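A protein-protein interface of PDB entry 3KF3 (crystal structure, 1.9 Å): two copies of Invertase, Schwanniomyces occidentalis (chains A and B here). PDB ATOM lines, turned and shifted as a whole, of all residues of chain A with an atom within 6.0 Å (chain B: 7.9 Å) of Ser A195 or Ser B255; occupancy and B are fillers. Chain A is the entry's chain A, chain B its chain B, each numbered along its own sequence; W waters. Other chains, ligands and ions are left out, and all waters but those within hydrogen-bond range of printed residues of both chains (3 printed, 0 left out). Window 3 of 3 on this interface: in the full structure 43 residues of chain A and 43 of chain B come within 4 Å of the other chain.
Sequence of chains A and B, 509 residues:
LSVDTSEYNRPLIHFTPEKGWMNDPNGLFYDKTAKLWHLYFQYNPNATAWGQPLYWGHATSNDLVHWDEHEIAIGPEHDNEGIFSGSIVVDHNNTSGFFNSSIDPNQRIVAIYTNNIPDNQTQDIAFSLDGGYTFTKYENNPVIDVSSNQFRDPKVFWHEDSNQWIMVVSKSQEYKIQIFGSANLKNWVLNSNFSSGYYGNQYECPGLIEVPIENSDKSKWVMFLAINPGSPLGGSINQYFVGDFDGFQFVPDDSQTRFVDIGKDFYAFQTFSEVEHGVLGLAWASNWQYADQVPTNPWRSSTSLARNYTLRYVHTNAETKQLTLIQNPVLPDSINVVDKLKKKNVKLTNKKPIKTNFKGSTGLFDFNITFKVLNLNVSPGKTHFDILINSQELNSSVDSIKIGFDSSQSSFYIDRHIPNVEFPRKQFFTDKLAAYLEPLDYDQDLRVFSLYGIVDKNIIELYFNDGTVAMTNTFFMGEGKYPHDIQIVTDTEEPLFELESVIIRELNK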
ATOM      1  N   GLU A 174       0.514 -10.332  -2.205  1.00  0.00           N
ATOM      2  CA  GLU A 174       1.322  -9.353  -1.475  1.00  0.00           C
ATOM      3  C   GLU A 174       1.849  -8.226  -2.366  1.00  0.00           C
ATOM      4  O   GLU A 174       2.458  -7.276  -1.876  1.00  0.00           O
ATOM      5  CB  GLU A 174       2.482 -10.037  -0.738  1.00  0.00           C
ATOM      6  CG  GLU A 174       2.041 -10.883   0.448  1.00  0.00           C
ATOM      7  CD  GLU A 174       3.204 -11.358   1.309  1.00  0.00           C
ATOM      8  OE1 GLU A 174       4.209 -10.625   1.437  1.00  0.00           O
ATOM      9  OE2 GLU A 174       3.107 -12.471   1.864  1.00  0.00           O
ATOM     10  N   TYR A 175       1.601  -8.324  -3.671  1.00  0.00           N
ATOM     11  CA  TYR A 175       2.101  -7.345  -4.642  1.00  0.00           C
ATOM     12  C   TYR A 175       3.620  -7.213  -4.566  1.00  0.00           C
ATOM     13  O   TYR A 175       4.159  -6.104  -4.469  1.00  0.00           O
ATOM     14  CB  TYR A 175       1.434  -5.970  -4.454  1.00  0.00           C
ATOM     15  CG  TYR A 175      -0.075  -5.983  -4.546  1.00  0.00           C
ATOM     16  CD1 TYR A 175      -0.861  -5.710  -3.431  1.00  0.00           C
ATOM     17  CD2 TYR A 175      -0.712  -6.262  -5.753  1.00  0.00           C
ATOM     18  CE1 TYR A 175      -2.248  -5.703  -3.514  1.00  0.00           C
ATOM     19  CE2 TYR A 175      -2.104  -6.267  -5.850  1.00  0.00           C
ATOM     20  CZ  TYR A 175      -2.861  -5.983  -4.732  1.00  0.00           C
ATOM     21  OH  TYR A 175      -4.226  -5.998  -4.833  1.00  0.00           O
ATOM     22  N   LYS A 176       4.305  -8.356  -4.595  1.00  0.00           N
ATOM     23  CA  LYS A 176       5.756  -8.386  -4.614  1.00  0.00           C
ATOM     24  C   LYS A 176       6.269  -9.369  -5.656  1.00  0.00           C
ATOM     25  O   LYS A 176       5.805 -10.507  -5.733  1.00  0.00           O
ATOM     26  CB  LYS A 176       6.307  -8.823  -3.254  1.00  0.00           C
ATOM     27  CG  LYS A 176       5.584  -8.239  -2.066  1.00  0.00           C
ATOM     28  CD  LYS A 176       6.439  -7.249  -1.341  1.00  0.00           C
ATOM     29  CE  LYS A 176       7.045  -7.890  -0.125  1.00  0.00           C
ATOM     30  NZ  LYS A 176       6.052  -8.025   0.965  1.00  0.00           N
ATOM     31  N   ILE A 177       7.215  -8.903  -6.461  1.00  0.00           N
ATOM     32  CA  ILE A 177       8.097  -9.787  -7.211  1.00  0.00           C
ATOM     33  C   ILE A 177       9.270 -10.059  -6.283  1.00  0.00           C
ATOM     34  O   ILE A 177       9.931  -9.134  -5.808  1.00  0.00           O
ATOM     35  CB  ILE A 177       8.586  -9.140  -8.515  1.00  0.00           C
ATOM     36  CG1 ILE A 177       7.395  -8.868  -9.441  1.00  0.00           C
ATOM     37  CG2 ILE A 177       9.641 -10.023  -9.212  1.00  0.00           C
ATOM     38  CD1 ILE A 177       7.719  -7.948 -10.594  1.00  0.00           C
ATOM     39  N   ASN A 193      12.775  -7.738  -2.620  1.00  0.00           N
ATOM     40  CA  ASN A 193      11.386  -7.630  -3.053  1.00  0.00           C
ATOM     41  C   ASN A 193      11.186  -6.374  -3.871  1.00  0.00           C
ATOM     42  O   ASN A 193      11.722  -5.317  -3.527  1.00  0.00           O
ATOM     43  CB  ASN A 193      10.455  -7.560  -1.849  1.00  0.00           C
ATOM     44  CG  ASN A 193      10.444  -8.827  -1.043  1.00  0.00           C
ATOM     45  OD1 ASN A 193      10.477  -9.937  -1.591  1.00  0.00           O
ATOM     46  ND2 ASN A 193      10.392  -8.672   0.281  1.00  0.00           N
ATOM     47  N   PHE A 194      10.403  -6.488  -4.944  1.00  0.00           N
ATOM     48  CA  PHE A 194      10.074  -5.340  -5.790  1.00  0.00           C
ATOM     49  C   PHE A 194       8.565  -5.174  -5.911  1.00  0.00           C
ATOM     50  O   PHE A 194       7.854  -6.131  -6.215  1.00  0.00           O
ATOM     51  CB  PHE A 194      10.698  -5.492  -7.187  1.00  0.00           C
ATOM     52  CG  PHE A 194      10.428  -4.325  -8.110  1.00  0.00           C
ATOM     53  CD1 PHE A 194      11.113  -3.119  -7.955  1.00  0.00           C
ATOM     54  CD2 PHE A 194       9.499  -4.438  -9.145  1.00  0.00           C
ATOM     55  CE1 PHE A 194      10.866  -2.038  -8.815  1.00  0.00           C
ATOM     56  CE2 PHE A 194       9.245  -3.363 -10.008  1.00  0.00           C
ATOM     57  CZ  PHE A 194       9.934  -2.165  -9.845  1.00  0.00           C
ATOM     58  N   SER A 195       8.095  -3.949  -5.683  1.00  0.00           N
ATOM     59  CA  SER A 195       6.670  -3.609  -5.750  1.00  0.00           C
ATOM     60  C   SER A 195       6.514  -2.264  -6.441  1.00  0.00           C
ATOM     61  O   SER A 195       7.085  -1.272  -5.987  1.00  0.00           O
ATOM     62  CB  SER A 195       6.085  -3.500  -4.347  1.00  0.00           C
ATOM     63  OG  SER A 195       6.255  -4.702  -3.629  1.00  0.00           O
ATOM     64  N   SER A 196       5.753  -2.230  -7.536  1.00  0.00           N
ATOM     65  CA  SER A 196       5.525  -0.984  -8.283  1.00  0.00           C
ATOM     66  C   SER A 196       4.416  -1.135  -9.321  1.00  0.00           C
ATOM     67  O   SER A 196       3.779  -2.189  -9.408  1.00  0.00           O
ATOM     68  CB  SER A 196       6.815  -0.508  -8.965  1.00  0.00           C
ATOM     69  OG  SER A 196       6.679   0.823  -9.445  1.00  0.00           O
ATOM     70  N   GLY A 197       4.179  -0.065 -10.078  1.00  0.00           N
ATOM     71  CA  GLY A 197       3.310  -0.099 -11.255  1.00  0.00           C
ATOM     72  C   GLY A 197       1.832  -0.200 -10.946  1.00  0.00           C
ATOM     73  O   GLY A 197       1.373   0.253  -9.898  1.00  0.00           O
ATOM     74  N   TYR A 199      -1.121  -2.215  -9.692  1.00  0.00           N
ATOM     75  CA  TYR A 199      -1.228  -3.395  -8.824  1.00  0.00           C
ATOM     76  C   TYR A 199      -2.329  -4.354  -9.253  1.00  0.00           C
ATOM     77  O   TYR A 199      -2.146  -5.568  -9.211  1.00  0.00           O
ATOM     78  CB  TYR A 199      -1.476  -2.977  -7.370  1.00  0.00           C
ATOM     79  CG  TYR A 199      -0.258  -2.522  -6.579  1.00  0.00           C
ATOM     80  CD1 TYR A 199       0.946  -2.200  -7.204  1.00  0.00           C
ATOM     81  CD2 TYR A 199      -0.332  -2.392  -5.197  1.00  0.00           C
ATOM     82  CE1 TYR A 199       2.047  -1.776  -6.466  1.00  0.00           C
ATOM     83  CE2 TYR A 199       0.756  -1.957  -4.449  1.00  0.00           C
ATOM     84  CZ  TYR A 199       1.940  -1.656  -5.085  1.00  0.00           C
ATOM     85  OH  TYR A 199       3.013  -1.225  -4.334  1.00  0.00           O
ATOM     86  N   TYR A 203      -0.279  -9.880  -8.540  1.00  0.00           N
ATOM     87  CA  TYR A 203       0.926 -10.019  -9.360  1.00  0.00           C
ATOM     88  C   TYR A 203       1.029 -11.455  -9.876  1.00  0.00           C
ATOM     89  O   TYR A 203       0.848 -12.394  -9.109  1.00  0.00           O
ATOM     90  CB  TYR A 203       2.163  -9.771  -8.499  1.00  0.00           C
ATOM     91  CG  TYR A 203       2.596  -8.340  -8.329  1.00  0.00           C
ATOM     92  CD1 TYR A 203       1.712  -7.273  -8.519  1.00  0.00           C
ATOM     93  CD2 TYR A 203       3.904  -8.057  -7.947  1.00  0.00           C
ATOM     94  CE1 TYR A 203       2.142  -5.950  -8.341  1.00  0.00           C
ATOM     95  CE2 TYR A 203       4.338  -6.763  -7.774  1.00  0.00           C
ATOM     96  CZ  TYR A 203       3.457  -5.710  -7.968  1.00  0.00           C
ATOM     97  OH  TYR A 203       3.927  -4.426  -7.787  1.00  0.00           O
ATOM     98  N   SER A 255       9.754   5.848 -12.018  1.00  0.00           N
ATOM     99  CA  SER A 255       8.677   5.152 -11.335  1.00  0.00           C
ATOM    100  C   SER A 255       7.387   5.152 -12.155  1.00  0.00           C
ATOM    101  O   SER A 255       6.298   5.151 -11.592  1.00  0.00           O
ATOM    102  CB  SER A 255       8.457   5.749  -9.939  1.00  0.00           C
ATOM    103  OG  SER A 255       8.014   7.094 -10.015  1.00  0.00           O
ATOM    104  N   THR A 257       4.483   3.739 -14.895  1.00  0.00           N
ATOM    105  CA  THR A 257       3.779   2.512 -15.246  1.00  0.00           C
ATOM    106  C   THR A 257       3.593   2.447 -16.760  1.00  0.00           C
ATOM    107  O   THR A 257       3.127   3.410 -17.362  1.00  0.00           O
ATOM    108  CB  THR A 257       2.412   2.454 -14.526  1.00  0.00           C
ATOM    109  OG1 THR A 257       2.621   2.240 -13.121  1.00  0.00           O
ATOM    110  CG2 THR A 257       1.535   1.333 -15.074  1.00  0.00           C
ATOM    111  N   PHE B 194       8.138  16.463  -9.198  1.00  0.00           N
ATOM    112  CA  PHE B 194       7.612  15.121  -9.006  1.00  0.00           C
ATOM    113  C   PHE B 194       7.200  14.490 -10.338  1.00  0.00           C
ATOM    114  O   PHE B 194       6.462  15.096 -11.129  1.00  0.00           O
ATOM    115  CB  PHE B 194       6.453  15.118  -8.000  1.00  0.00           C
ATOM    116  CG  PHE B 194       5.926  13.744  -7.683  1.00  0.00           C
ATOM    117  CD1 PHE B 194       6.711  12.820  -6.995  1.00  0.00           C
ATOM    118  CD2 PHE B 194       4.643  13.372  -8.076  1.00  0.00           C
ATOM    119  CE1 PHE B 194       6.221  11.543  -6.705  1.00  0.00           C
ATOM    120  CE2 PHE B 194       4.143  12.099  -7.786  1.00  0.00           C
ATOM    121  CZ  PHE B 194       4.930  11.186  -7.101  1.00  0.00           C
ATOM    122  N   SER B 196       5.972  10.567 -11.793  1.00  0.00           N
ATOM    123  CA  SER B 196       5.546   9.204 -11.470  1.00  0.00           C
ATOM    124  C   SER B 196       4.263   8.800 -12.201  1.00  0.00           C
ATOM    125  O   SER B 196       3.669   9.605 -12.913  1.00  0.00           O
ATOM    126  CB  SER B 196       5.350   9.049  -9.961  1.00  0.00           C
ATOM    127  OG  SER B 196       5.247   7.683  -9.593  1.00  0.00           O
ATOM    128  N   GLY B 197       3.864   7.544 -12.020  1.00  0.00           N
ATOM    129  CA  GLY B 197       2.577   7.044 -12.490  1.00  0.00           C
ATOM    130  C   GLY B 197       2.488   6.779 -13.978  1.00  0.00           C
ATOM    131  O   GLY B 197       3.478   6.410 -14.619  1.00  0.00           O
ATOM    132  N   TYR B 198       1.288   6.963 -14.523  1.00  0.00           N
ATOM    133  CA  TYR B 198       1.052   6.822 -15.949  1.00  0.00           C
ATOM    134  C   TYR B 198       1.307   8.145 -16.662  1.00  0.00           C
ATOM    135  O   TYR B 198       0.605   9.129 -16.423  1.00  0.00           O
ATOM    136  CB  TYR B 198      -0.381   6.344 -16.216  1.00  0.00           C
ATOM    137  CG  TYR B 198      -0.496   5.505 -17.464  1.00  0.00           C
ATOM    138  CD1 TYR B 198      -0.230   4.137 -17.421  1.00  0.00           C
ATOM    139  CD2 TYR B 198      -0.851   6.069 -18.691  1.00  0.00           C
ATOM    140  CE1 TYR B 198      -0.317   3.349 -18.550  1.00  0.00           C
ATOM    141  CE2 TYR B 198      -0.942   5.278 -19.845  1.00  0.00           C
ATOM    142  CZ  TYR B 198      -0.676   3.914 -19.756  1.00  0.00           C
ATOM    143  OH  TYR B 198      -0.757   3.094 -20.858  1.00  0.00           O
ATOM    144  N   PHE B 241      -1.748   9.906  -6.184  1.00  0.00           N
ATOM    145  CA  PHE B 241      -0.648   9.333  -5.419  1.00  0.00           C
ATOM    146  C   PHE B 241      -0.844   9.694  -3.948  1.00  0.00           C
ATOM    147  O   PHE B 241      -1.226  10.813  -3.636  1.00  0.00           O
ATOM    148  CB  PHE B 241       0.697   9.917  -5.871  1.00  0.00           C
ATOM    149  CG  PHE B 241       0.913   9.912  -7.357  1.00  0.00           C
ATOM    150  CD1 PHE B 241       1.594   8.866  -7.970  1.00  0.00           C
ATOM    151  CD2 PHE B 241       0.469  10.968  -8.142  1.00  0.00           C
ATOM    152  CE1 PHE B 241       1.801   8.862  -9.353  1.00  0.00           C
ATOM    153  CE2 PHE B 241       0.680  10.984  -9.516  1.00  0.00           C
ATOM    154  CZ  PHE B 241       1.347   9.932 -10.128  1.00  0.00           C
ATOM    155  N   VAL B 242      -0.547   8.761  -3.053  1.00  0.00           N
ATOM    156  CA  VAL B 242      -0.752   8.965  -1.626  1.00  0.00           C
ATOM    157  C   VAL B 242       0.607   9.007  -0.938  1.00  0.00           C
ATOM    158  O   VAL B 242       1.459   8.138  -1.171  1.00  0.00           O
ATOM    159  CB  VAL B 242      -1.635   7.849  -1.023  1.00  0.00           C
ATOM    160  CG1 VAL B 242      -1.830   8.036   0.492  1.00  0.00           C
ATOM    161  CG2 VAL B 242      -2.985   7.801  -1.733  1.00  0.00           C
ATOM    162  N   PRO B 252       5.668  10.033  -2.041  1.00  0.00           N
ATOM    163  CA  PRO B 252       4.629   9.006  -2.043  1.00  0.00           C
ATOM    164  C   PRO B 252       4.995   7.843  -1.131  1.00  0.00           C
ATOM    165  O   PRO B 252       6.187   7.572  -0.923  1.00  0.00           O
ATOM    166  CB  PRO B 252       4.571   8.556  -3.505  1.00  0.00           C
ATOM    167  CG  PRO B 252       5.860   8.947  -4.095  1.00  0.00           C
ATOM    168  CD  PRO B 252       6.332  10.160  -3.352  1.00  0.00           C
ATOM    169  N   ASP B 253       3.976   7.181  -0.589  1.00  0.00           N
ATOM    170  CA  ASP B 253       4.152   6.021   0.280  1.00  0.00           C
ATOM    171  C   ASP B 253       4.577   4.785  -0.497  1.00  0.00           C
ATOM    172  O   ASP B 253       5.164   3.864   0.065  1.00  0.00           O
ATOM    173  CB  ASP B 253       2.856   5.710   1.018  1.00  0.00           C
ATOM    174  CG  ASP B 253       2.567   6.686   2.151  1.00  0.00           C
ATOM    175  OD1 ASP B 253       3.468   7.460   2.555  1.00  0.00           O
ATOM    176  OD2 ASP B 253       1.425   6.655   2.647  1.00  0.00           O
ATOM    177  N   ASP B 254       4.257   4.769  -1.788  1.00  0.00           N
ATOM    178  CA  ASP B 254       4.627   3.675  -2.676  1.00  0.00           C
ATOM    179  C   ASP B 254       4.836   4.253  -4.063  1.00  0.00           C
ATOM    180  O   ASP B 254       4.762   5.468  -4.247  1.00  0.00           O
ATOM    181  CB  ASP B 254       3.539   2.587  -2.681  1.00  0.00           C
ATOM    182  CG  ASP B 254       2.147   3.135  -3.011  1.00  0.00           C
ATOM    183  OD1 ASP B 254       1.158   2.611  -2.461  1.00  0.00           O
ATOM    184  OD2 ASP B 254       2.034   4.089  -3.812  1.00  0.00           O
ATOM    185  N   SER B 255       5.086   3.394  -5.044  1.00  0.00           N
ATOM    186  CA  SER B 255       5.246   3.851  -6.417  1.00  0.00           C
ATOM    187  C   SER B 255       4.177   3.262  -7.346  1.00  0.00           C
ATOM    188  O   SER B 255       4.428   3.071  -8.533  1.00  0.00           O
ATOM    189  CB  SER B 255       6.661   3.538  -6.931  1.00  0.00           C
ATOM    190  OG  SER B 255       6.881   2.139  -6.974  1.00  0.00           O
ATOM    191  N   GLN B 256       2.988   2.990  -6.805  1.00  0.00           N
ATOM    192  CA  GLN B 256       1.888   2.440  -7.605  1.00  0.00           C
ATOM    193  C   GLN B 256       1.070   3.527  -8.315  1.00  0.00           C
ATOM    194  O   GLN B 256       1.008   4.677  -7.861  1.00  0.00           O
ATOM    195  CB  GLN B 256       0.980   1.533  -6.762  1.00  0.00           C
ATOM    196  CG  GLN B 256      -0.053   2.254  -5.907  1.00  0.00           C
ATOM    197  CD  GLN B 256      -1.021   1.300  -5.250  1.00  0.00           C
ATOM    198  OE1 GLN B 256      -1.804   0.630  -5.922  1.00  0.00           O
ATOM    199  NE2 GLN B 256      -0.965   1.223  -3.927  1.00  0.00           N
ATOM    200  N   THR B 257       0.452   3.132  -9.426  1.00  0.00           N
ATOM    201  CA  THR B 257      -0.400   3.990 -10.242  1.00  0.00           C
ATOM    202  C   THR B 257      -1.860   3.642  -9.978  1.00  0.00           C
ATOM    203  O   THR B 257      -2.244   2.475 -10.049  1.00  0.00           O
ATOM    204  CB  THR B 257      -0.087   3.782 -11.745  1.00  0.00           C
ATOM    205  OG1 THR B 257       1.199   4.342 -12.037  1.00  0.00           O
ATOM    206  CG2 THR B 257      -1.140   4.445 -12.640  1.00  0.00           C
ATOM    207  N   ARG B 258      -2.668   4.650  -9.655  1.00  0.00           N
ATOM    208  CA  ARG B 258      -4.108   4.457  -9.478  1.00  0.00           C
ATOM    209  C   ARG B 258      -4.883   5.622 -10.081  1.00  0.00           C
ATOM    210  O   ARG B 258      -4.446   6.761  -9.998  1.00  0.00           O
ATOM    211  CB  ARG B 258      -4.464   4.307  -7.996  1.00  0.00           C
ATOM    212  CG  ARG B 258      -3.892   3.072  -7.342  1.00  0.00           C
ATOM    213  CD  ARG B 258      -4.167   3.056  -5.861  1.00  0.00           C
ATOM    214  NE  ARG B 258      -3.250   3.919  -5.109  1.00  0.00           N
ATOM    215  CZ  ARG B 258      -3.232   3.979  -3.783  1.00  0.00           C
ATOM    216  NH1 ARG B 258      -4.080   3.233  -3.083  1.00  0.00           N
ATOM    217  NH2 ARG B 258      -2.370   4.770  -3.151  1.00  0.00           N
HETATM  218  O   HOH W   1       5.132   0.275  -4.676  1.00  0.00           O
HETATM  219  O   HOH W   2       4.007   3.785 -11.238  1.00  0.00           O
HETATM  220  O   HOH W   3      -2.270   0.167  -8.600  1.00  0.00           O
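O of Gly A197 sits at hydrogen-bond distance from N of Thr B257 (3.1 Å). OG of Ser A196 is in hydrogen-bond range of OG of Ser B255 (2.8 Å). OG1 of Thr B257 sits at hydrogen-bond distance from OG1 of Thr A257 (2.8 Å). The backbone carbonyl oxygen (O) of Ser A255 lies within hydrogen-bond range of the backbone NH (N) of Gly B197 (3.4 Å). O of Gly B197 sits at hydrogen-bond distance from N of Thr A257 (2.9 Å). OG of Ser A255 is in hydrogen-bond range of OG of Ser B196, at 2.9 Å.
OH of Tyr A203 is in hydrogen-bond range of O of Ser A196. NE2 of Gln B256 lies within hydrogen-bond range of OD1 of Asp B254, at 2.9 Å. O of Tyr A175 sits at hydrogen-bond distance from OG of Ser A195 (2.7 Å).
Ser B255 touches Ser A195 (OG to O, 3.6 Å). Gly A197 touches Ser B255. Gln B256 touches Gly A197 (CA to O, 3.2 Å). OE1 of Gln B256 touches CD2 of Tyr A199, at 3.4 Å. Tyr B198 touches Thr A257.
Of the printed residues of chain B, Ser A195 touches Ser B255 (3.6 Å). Of the printed residues of chain B, Gly A197 touches Ser B255 (3.5 Å), Gln B256 (3.2 Å) and Thr B257 (3.1 Å). Of the printed residues of chain B, Thr A257 touches Gly B197 (2.9 Å), Tyr B198 (3.4 Å) and Thr B257 (2.8 Å). Of the printed residues of chain A, Ser B196 touches Ser A255 (2.9 Å). Of the printed residues of chain A, Gln B256 touches Gly A197 (3.2 Å) and Tyr A199 (3.4 Å). Phe B241 touches none of the printed residues of chain A. Tyr A175 touches none of the printed residues of chain B. The nearest residue of chain B that does not touch Ser A195 is Gln B256 (6.0 Å).
Hydrophobic or aromatic side chains of chain A within 4 Å of the printed part of chain B: Tyr A199. Of the 13 printed residues of chain B, 6 touch a printed residue of chain A. Along chain B the printed residues that touch a printed residue of chain A span positions 196 to 257. Among the printed residues, no Asp or Glu carboxylate lies within 4 Å of a Lys or Arg side-chain nitrogen of the other chain.
Ser A196 touches Ser B255, and with the chains exchanged Ser A255 touches Ser B196. Gly A197 touches Ser B255, and with the chains exchanged Ser A255 touches Gly B197. Gly A197 touches Thr B257, and with the chains exchanged Thr A257 touches Gly B197. Thr B257 touches its own counterpart, Thr A257. 5 positions are printed for both chains.
Water W1 lies within hydrogen-bond range of OH of Tyr A199, O of Ser A195 and N of Ser B255. Water W2 lies within hydrogen-bond range of the backbone carbonyl oxygen (O) of Ser A255 (2.7 Å), the side-chain hydroxyl (OG1) of Thr A257 (2.8 Å), the backbone carbonyl oxygen (O) of Ser B255 (2.8 Å) and the side-chain hydroxyl (OG1) of Thr B257 (3.0 Å). Water W3 lies within hydrogen-bond range of the backbone carbonyl oxygen (O) of Thr B257 (2.7 Å), the side-chain amide oxygen (OE1) of Gln B256 (2.8 Å) and the backbone NH (N) of Tyr A199 (2.9 Å).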
